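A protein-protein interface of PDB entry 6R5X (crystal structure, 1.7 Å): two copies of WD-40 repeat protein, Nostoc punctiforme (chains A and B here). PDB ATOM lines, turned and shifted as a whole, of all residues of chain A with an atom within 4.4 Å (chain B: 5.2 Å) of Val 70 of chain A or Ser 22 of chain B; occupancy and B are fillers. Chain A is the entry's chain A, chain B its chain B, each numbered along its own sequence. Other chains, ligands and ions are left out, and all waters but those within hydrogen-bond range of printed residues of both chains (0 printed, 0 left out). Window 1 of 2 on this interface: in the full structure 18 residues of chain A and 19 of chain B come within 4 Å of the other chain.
Ala 64 of chain A touches none of the printed residues of chain B. Of chain B, only Ser 22 comes within 4 Å of Val 70 of chain A. Of the printed residues of chain A, Gly 10 of chain B touches Trp 50. Ser 22 of chain B touches just these residues of chain A: Trp 50 (3.7 Å) and Val 70 (3.9 Å). Printed residues of chain A within 4 Å of Trp 32 of chain B: Leu 83. The nearest residue of chain B that does not touch Val 70 of chain A is Trp 32 of chain B (4.03 Å). The nearest residue of chain A that does not touch Ser 22 of chain B is Ala 64 of chain A (4.2 Å). The nearest printed residue of chain A that does not touch Gly 10 of chain B is Ala 64 of chain A (5.7 Å).
CH2 of Trp 50 of chain A touches O of Gly 10 of chain B, at 3.7 Å. Trp 50 of chain A touches Ser 22 of chain B. O of Ala 23 of chain B touches CZ2 of Trp 50 of chain A (3.9 Å). Val 70 of chain A touches Ser 22 of chain B. Leu 72 of chain A touches Ile 20 of chain B. CB of Leu 83 of chain A touches CE2 of Trp 32 of chain B, at 3.6 Å.
The backbone NH of Leu 83 of chain A lies within hydrogen-bond range of the backbone carbonyl oxygen of Val 70 of chain A, 2.7 Å away. The backbone NH of Leu 72 of chain A is in hydrogen-bond range of the backbone carbonyl oxygen of Gln 81 of chain A (2.9 Å). The side-chain hydroxyl of Ser 22 of chain B sits at hydrogen-bond distance from the backbone carbonyl oxygen of Gly 10 of chain B (3.3 Å). N of Ala 23 of chain B sits at hydrogen-bond distance from O of Gly 10 of chain B (2.9 Å). N of Ile 20 of chain B sits at hydrogen-bond distance from O of Trp 32 of chain B (2.9 Å). The backbone NH (N) of Ser 22 of chain B is in hydrogen-bond range of the backbone carbonyl oxygen (O) of Lys 30 of chain B, 3.0 Å away.
Of the 11 printed residues of chain A, 4 touch a printed residue of chain B. Printed residues of chain A that touch a printed residue of chain B: Trp 50, Val 70, Leu 72 and Leu 83. Hydrophobic or aromatic side chains of chain A that line the printed part of chain B: Trp 50, Val 70, Leu 72 and Leu 83. Printed residues of chain B that touch a printed residue of chain A: Gly 10, Ile 20, Ser 22, Ala 23 and Trp 32. Among the printed residues, 6 pairs touch across the chains.
No position is printed for both chains. Of the 6 pairs that touch across the chains among the printed residues, none has its exchanged pair printed and touching as well.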
ATOM      1  N   TRP A  50      26.153 -30.530 -15.845  1.00  0.00           N
ATOM      2  CA  TRP A  50      24.757 -30.469 -16.302  1.00  0.00           C
ATOM      3  C   TRP A  50      24.090 -29.092 -16.207  1.00  0.00           C
ATOM      4  O   TRP A  50      23.057 -28.880 -16.860  1.00  0.00           O
ATOM      5  CB  TRP A  50      23.865 -31.497 -15.599  1.00  0.00           C
ATOM      6  CG  TRP A  50      23.907 -31.526 -14.060  1.00  0.00           C
ATOM      7  CD1 TRP A  50      24.569 -32.422 -13.288  1.00  0.00           C
ATOM      8  CD2 TRP A  50      23.208 -30.663 -13.150  1.00  0.00           C
ATOM      9  NE1 TRP A  50      24.349 -32.180 -11.955  1.00  0.00           N
ATOM     10  CE2 TRP A  50      23.502 -31.107 -11.843  1.00  0.00           C
ATOM     11  CE3 TRP A  50      22.361 -29.564 -13.316  1.00  0.00           C
ATOM     12  CZ2 TRP A  50      22.997 -30.471 -10.703  1.00  0.00           C
ATOM     13  CZ3 TRP A  50      21.880 -28.913 -12.176  1.00  0.00           C
ATOM     14  CH2 TRP A  50      22.189 -29.378 -10.890  1.00  0.00           C
ATOM     15  N   ALA A  62      28.411 -20.122 -12.016  1.00  0.00           N
ATOM     16  CA  ALA A  62      28.287 -21.363 -11.269  1.00  0.00           C
ATOM     17  C   ALA A  62      28.107 -22.568 -12.224  1.00  0.00           C
ATOM     18  O   ALA A  62      27.409 -22.467 -13.256  1.00  0.00           O
ATOM     19  CB  ALA A  62      27.134 -21.270 -10.329  1.00  0.00           C
ATOM     20  N   SER A  63      28.774 -23.665 -11.915  1.00  0.00           N
ATOM     21  CA  SER A  63      28.667 -24.886 -12.679  1.00  0.00           C
ATOM     22  C   SER A  63      28.305 -26.046 -11.741  1.00  0.00           C
ATOM     23  O   SER A  63      28.853 -26.177 -10.656  1.00  0.00           O
ATOM     24  CB  SER A  63      29.956 -25.181 -13.433  1.00  0.00           C
ATOM     25  OG  SER A  63      31.097 -25.237 -12.580  1.00  0.00           O
ATOM     26  N   ALA A  64      27.329 -26.853 -12.139  1.00  0.00           N
ATOM     27  CA  ALA A  64      26.859 -27.967 -11.322  1.00  0.00           C
ATOM     28  C   ALA A  64      27.103 -29.249 -12.077  1.00  0.00           C
ATOM     29  O   ALA A  64      26.774 -29.358 -13.265  1.00  0.00           O
ATOM     30  CB  ALA A  64      25.380 -27.814 -11.013  1.00  0.00           C
ATOM     31  N   THR A  69      29.353 -31.585  -6.939  1.00  0.00           N
ATOM     32  CA  THR A  69      29.800 -30.273  -6.499  1.00  0.00           C
ATOM     33  C   THR A  69      29.170 -29.182  -7.361  1.00  0.00           C
ATOM     34  O   THR A  69      28.709 -29.429  -8.483  1.00  0.00           O
ATOM     35  CB  THR A  69      31.335 -30.113  -6.562  1.00  0.00           C
ATOM     36  OG1 THR A  69      31.769 -30.032  -7.928  1.00  0.00           O
ATOM     37  CG2 THR A  69      32.043 -31.239  -5.868  1.00  0.00           C
ATOM     38  N   VAL A  70      29.168 -27.962  -6.823  1.00  0.00           N
ATOM     39  CA  VAL A  70      28.885 -26.744  -7.560  1.00  0.00           C
ATOM     40  C   VAL A  70      30.139 -25.874  -7.452  1.00  0.00           C
ATOM     41  O   VAL A  70      30.604 -25.621  -6.360  1.00  0.00           O
ATOM     42  CB  VAL A  70      27.680 -25.961  -6.999  1.00  0.00           C
ATOM     43  CG1 VAL A  70      27.479 -24.655  -7.757  1.00  0.00           C
ATOM     44  CG2 VAL A  70      26.408 -26.806  -7.045  1.00  0.00           C
ATOM     45  N   LYS A  71      30.727 -25.490  -8.578  1.00  0.00           N
ATOM     46  CA  LYS A  71      31.913 -24.658  -8.555  1.00  0.00           C
ATOM     47  C   LYS A  71      31.529 -23.219  -8.958  1.00  0.00           C
ATOM     48  O   LYS A  71      30.671 -23.018  -9.818  1.00  0.00           O
ATOM     49  CB  LYS A  71      33.020 -25.233  -9.443  1.00  0.00           C
ATOM     50  CG  LYS A  71      33.685 -26.453  -8.824  1.00  0.00           C
ATOM     51  CD  LYS A  71      34.633 -27.169  -9.780  1.00  0.00           C
ATOM     52  CE  LYS A  71      35.159 -28.493  -9.214  1.00  0.00           C
ATOM     53  NZ  LYS A  71      36.180 -28.338  -8.139  1.00  0.00           N
ATOM     54  N   LEU A  72      32.175 -22.264  -8.306  1.00  0.00           N
ATOM     55  CA  LEU A  72      32.023 -20.831  -8.589  1.00  0.00           C
ATOM     56  C   LEU A  72      33.312 -20.311  -9.178  1.00  0.00           C
ATOM     57  O   LEU A  72      34.401 -20.566  -8.624  1.00  0.00           O
ATOM     58  CB  LEU A  72      31.674 -20.057  -7.317  1.00  0.00           C
ATOM     59  CG  LEU A  72      30.443 -20.529  -6.555  1.00  0.00           C
ATOM     60  CD1 LEU A  72      30.190 -19.594  -5.386  1.00  0.00           C
ATOM     61  CD2 LEU A  72      29.217 -20.626  -7.444  1.00  0.00           C
ATOM     62  N   GLN A  81      35.413 -21.077  -5.520  1.00  0.00           N
ATOM     63  CA  GLN A  81      34.878 -21.957  -4.468  1.00  0.00           C
ATOM     64  C   GLN A  81      34.402 -23.275  -5.078  1.00  0.00           C
ATOM     65  O   GLN A  81      33.961 -23.308  -6.222  1.00  0.00           O
ATOM     66  CB  GLN A  81      33.644 -21.355  -3.771  1.00  0.00           C
ATOM     67  CG  GLN A  81      33.808 -20.016  -3.114  1.00  0.00           C
ATOM     68  CD  GLN A  81      34.699 -20.036  -1.897  1.00  0.00           C
ATOM     69  OE1 GLN A  81      34.990 -21.079  -1.309  1.00  0.00           O
ATOM     70  NE2 GLN A  81      35.140 -18.855  -1.499  1.00  0.00           N
ATOM     71  N   THR A  82      34.488 -24.342  -4.281  1.00  0.00           N
ATOM     72  CA  THR A  82      33.830 -25.620  -4.590  1.00  0.00           C
ATOM     73  C   THR A  82      32.825 -25.913  -3.466  1.00  0.00           C
ATOM     74  O   THR A  82      33.219 -26.163  -2.319  1.00  0.00           O
ATOM     75  CB  THR A  82      34.885 -26.748  -4.747  1.00  0.00           C
ATOM     76  OG1 THR A  82      35.783 -26.401  -5.812  1.00  0.00           O
ATOM     77  CG2 THR A  82      34.227 -28.072  -5.075  1.00  0.00           C
ATOM     78  N   LEU A  83      31.527 -25.875  -3.802  1.00  0.00           N
ATOM     79  CA  LEU A  83      30.453 -26.091  -2.812  1.00  0.00           C
ATOM     80  C   LEU A  83      30.053 -27.548  -2.802  1.00  0.00           C
ATOM     81  O   LEU A  83      29.825 -28.159  -3.849  1.00  0.00           O
ATOM     82  CB  LEU A  83      29.207 -25.297  -3.164  1.00  0.00           C
ATOM     83  CG  LEU A  83      29.383 -23.814  -3.453  1.00  0.00           C
ATOM     84  CD1 LEU A  83      28.090 -23.175  -3.899  1.00  0.00           C
ATOM     85  CD2 LEU A  83      29.942 -23.133  -2.230  1.00  0.00           C
ATOM     86  N   GLY B  10      18.388 -25.823 -12.935  1.00  0.00           N
ATOM     87  CA  GLY B  10      18.805 -26.724 -11.814  1.00  0.00           C
ATOM     88  C   GLY B  10      19.759 -26.105 -10.820  1.00  0.00           C
ATOM     89  O   GLY B  10      20.002 -26.652  -9.718  1.00  0.00           O
ATOM     90  N   VAL B  11      20.238 -24.914 -11.182  1.00  0.00           N
ATOM     91  CA  VAL B  11      21.187 -24.143 -10.349  1.00  0.00           C
ATOM     92  C   VAL B  11      20.909 -22.648 -10.581  1.00  0.00           C
ATOM     93  O   VAL B  11      20.654 -22.249 -11.729  1.00  0.00           O
ATOM     94  CB  VAL B  11      22.695 -24.511 -10.613  1.00  0.00           C
ATOM     95  CG1 VAL B  11      23.126 -24.282 -12.051  1.00  0.00           C
ATOM     96  CG2 VAL B  11      23.666 -23.762  -9.683  1.00  0.00           C
ATOM     97  N   ALA B  12      20.901 -21.851  -9.515  1.00  0.00           N
ATOM     98  CA  ALA B  12      20.606 -20.398  -9.636  1.00  0.00           C
ATOM     99  C   ALA B  12      21.299 -19.572  -8.560  1.00  0.00           C
ATOM    100  O   ALA B  12      21.503 -20.051  -7.443  1.00  0.00           O
ATOM    101  CB  ALA B  12      19.109 -20.117  -9.618  1.00  0.00           C
ATOM    102  N   ILE B  20      23.444 -19.222  -3.419  1.00  0.00           N
ATOM    103  CA  ILE B  20      23.385 -20.129  -4.570  1.00  0.00           C
ATOM    104  C   ILE B  20      22.437 -21.276  -4.180  1.00  0.00           C
ATOM    105  O   ILE B  20      22.560 -21.853  -3.083  1.00  0.00           O
ATOM    106  CB  ILE B  20      24.764 -20.686  -4.946  1.00  0.00           C
ATOM    107  CG1 ILE B  20      25.709 -19.561  -5.396  1.00  0.00           C
ATOM    108  CG2 ILE B  20      24.644 -21.734  -6.055  1.00  0.00           C
ATOM    109  CD1 ILE B  20      26.461 -18.891  -4.265  1.00  0.00           C
ATOM    110  N   ALA B  21      21.499 -21.597  -5.065  1.00  0.00           N
ATOM    111  CA  ALA B  21      20.594 -22.776  -4.871  1.00  0.00           C
ATOM    112  C   ALA B  21      20.914 -23.837  -5.911  1.00  0.00           C
ATOM    113  O   ALA B  21      21.139 -23.517  -7.086  1.00  0.00           O
ATOM    114  CB  ALA B  21      19.125 -22.418  -4.980  1.00  0.00           C
ATOM    115  N   SER B  22      20.925 -25.112  -5.506  1.00  0.00           N
ATOM    116  CA  SER B  22      21.045 -26.178  -6.491  1.00  0.00           C
ATOM    117  C   SER B  22      20.195 -27.391  -6.148  1.00  0.00           C
ATOM    118  O   SER B  22      20.044 -27.718  -4.973  1.00  0.00           O
ATOM    119  CB  SER B  22      22.493 -26.624  -6.628  1.00  0.00           C
ATOM    120  OG  SER B  22      22.639 -27.400  -7.793  1.00  0.00           O
ATOM    121  N   ALA B  23      19.705 -28.077  -7.170  1.00  0.00           N
ATOM    122  CA  ALA B  23      19.071 -29.365  -6.957  1.00  0.00           C
ATOM    123  C   ALA B  23      20.133 -30.420  -6.629  1.00  0.00           C
ATOM    124  O   ALA B  23      21.136 -30.535  -7.331  1.00  0.00           O
ATOM    125  CB  ALA B  23      18.292 -29.771  -8.170  1.00  0.00           C
ATOM    126  N   SER B  24      19.929 -31.169  -5.552  1.00  0.00           N
ATOM    127  CA  SER B  24      20.886 -32.200  -5.138  1.00  0.00           C
ATOM    128  C   SER B  24      20.328 -33.571  -5.542  1.00  0.00           C
ATOM    129  O   SER B  24      19.116 -33.755  -5.680  1.00  0.00           O
ATOM    130  CB  SER B  24      21.181 -32.102  -3.632  1.00  0.00           C
ATOM    131  OG  SER B  24      21.950 -33.207  -3.175  1.00  0.00           O
ATOM    132  N   THR B  28      16.758 -33.302  -2.386  1.00  0.00           N
ATOM    133  CA  THR B  28      16.746 -32.026  -1.639  1.00  0.00           C
ATOM    134  C   THR B  28      17.222 -30.860  -2.494  1.00  0.00           C
ATOM    135  O   THR B  28      17.794 -31.043  -3.568  1.00  0.00           O
ATOM    136  CB  THR B  28      17.650 -32.108  -0.375  1.00  0.00           C
ATOM    137  OG1 THR B  28      19.028 -32.214  -0.755  1.00  0.00           O
ATOM    138  CG2 THR B  28      17.279 -33.261   0.513  1.00  0.00           C
ATOM    139  N   VAL B  29      17.003 -29.653  -1.993  1.00  0.00           N
ATOM    140  CA  VAL B  29      17.618 -28.442  -2.546  1.00  0.00           C
ATOM    141  C   VAL B  29      18.603 -27.925  -1.518  1.00  0.00           C
ATOM    142  O   VAL B  29      18.245 -27.780  -0.341  1.00  0.00           O
ATOM    143  CB  VAL B  29      16.571 -27.358  -2.854  1.00  0.00           C
ATOM    144  CG1 VAL B  29      17.237 -26.057  -3.260  1.00  0.00           C
ATOM    145  CG2 VAL B  29      15.630 -27.848  -3.940  1.00  0.00           C
ATOM    146  N   LYS B  30      19.813 -27.582  -1.969  1.00  0.00           N
ATOM    147  CA  LYS B  30      20.819 -27.003  -1.096  1.00  0.00           C
ATOM    148  C   LYS B  30      20.931 -25.498  -1.356  1.00  0.00           C
ATOM    149  O   LYS B  30      20.894 -25.052  -2.517  1.00  0.00           O
ATOM    150  CB  LYS B  30      22.202 -27.636  -1.325  1.00  0.00           C
ATOM    151  CG  LYS B  30      22.286 -29.127  -1.102  1.00  0.00           C
ATOM    152  CD  LYS B  30      22.266 -29.545   0.358  1.00  0.00           C
ATOM    153  CE  LYS B  30      22.211 -31.057   0.582  1.00  0.00           C
ATOM    154  NZ  LYS B  30      22.443 -31.364   2.030  1.00  0.00           N
ATOM    155  N   TRP B  32      23.594 -22.339  -0.417  1.00  0.00           N
ATOM    156  CA  TRP B  32      24.919 -21.973   0.101  1.00  0.00           C
ATOM    157  C   TRP B  32      25.122 -20.453   0.047  1.00  0.00           C
ATOM    158  O   TRP B  32      24.522 -19.757  -0.803  1.00  0.00           O
ATOM    159  CB  TRP B  32      26.042 -22.549  -0.753  1.00  0.00           C
ATOM    160  CG  TRP B  32      26.256 -24.048  -0.753  1.00  0.00           C
ATOM    161  CD1 TRP B  32      27.049 -24.788   0.080  1.00  0.00           C
ATOM    162  CD2 TRP B  32      25.730 -24.952  -1.716  1.00  0.00           C
ATOM    163  NE1 TRP B  32      26.990 -26.119  -0.284  1.00  0.00           N
ATOM    164  CE2 TRP B  32      26.201 -26.232  -1.399  1.00  0.00           C
ATOM    165  CE3 TRP B  32      24.900 -24.785  -2.824  1.00  0.00           C
ATOM    166  CZ2 TRP B  32      25.874 -27.357  -2.168  1.00  0.00           C
ATOM    167  CZ3 TRP B  32      24.570 -25.901  -3.572  1.00  0.00           C
ATOM    168  CH2 TRP B  32      25.056 -27.157  -3.251  1.00  0.00           C
ATOM    169  N   VAL B  52      15.069 -25.197  -9.636  1.00  0.00           N
ATOM    170  CA  VAL B  52      14.982 -24.227  -8.539  1.00  0.00           C
ATOM    171  C   VAL B  52      14.881 -22.795  -9.093  1.00  0.00           C
ATOM    172  O   VAL B  52      15.384 -22.506 -10.193  1.00  0.00           O
ATOM    173  CB  VAL B  52      16.213 -24.304  -7.610  1.00  0.00           C
ATOM    174  CG1 VAL B  52      16.261 -25.669  -6.975  1.00  0.00           C
ATOM    175  CG2 VAL B  52      17.519 -24.024  -8.356  1.00  0.00           C
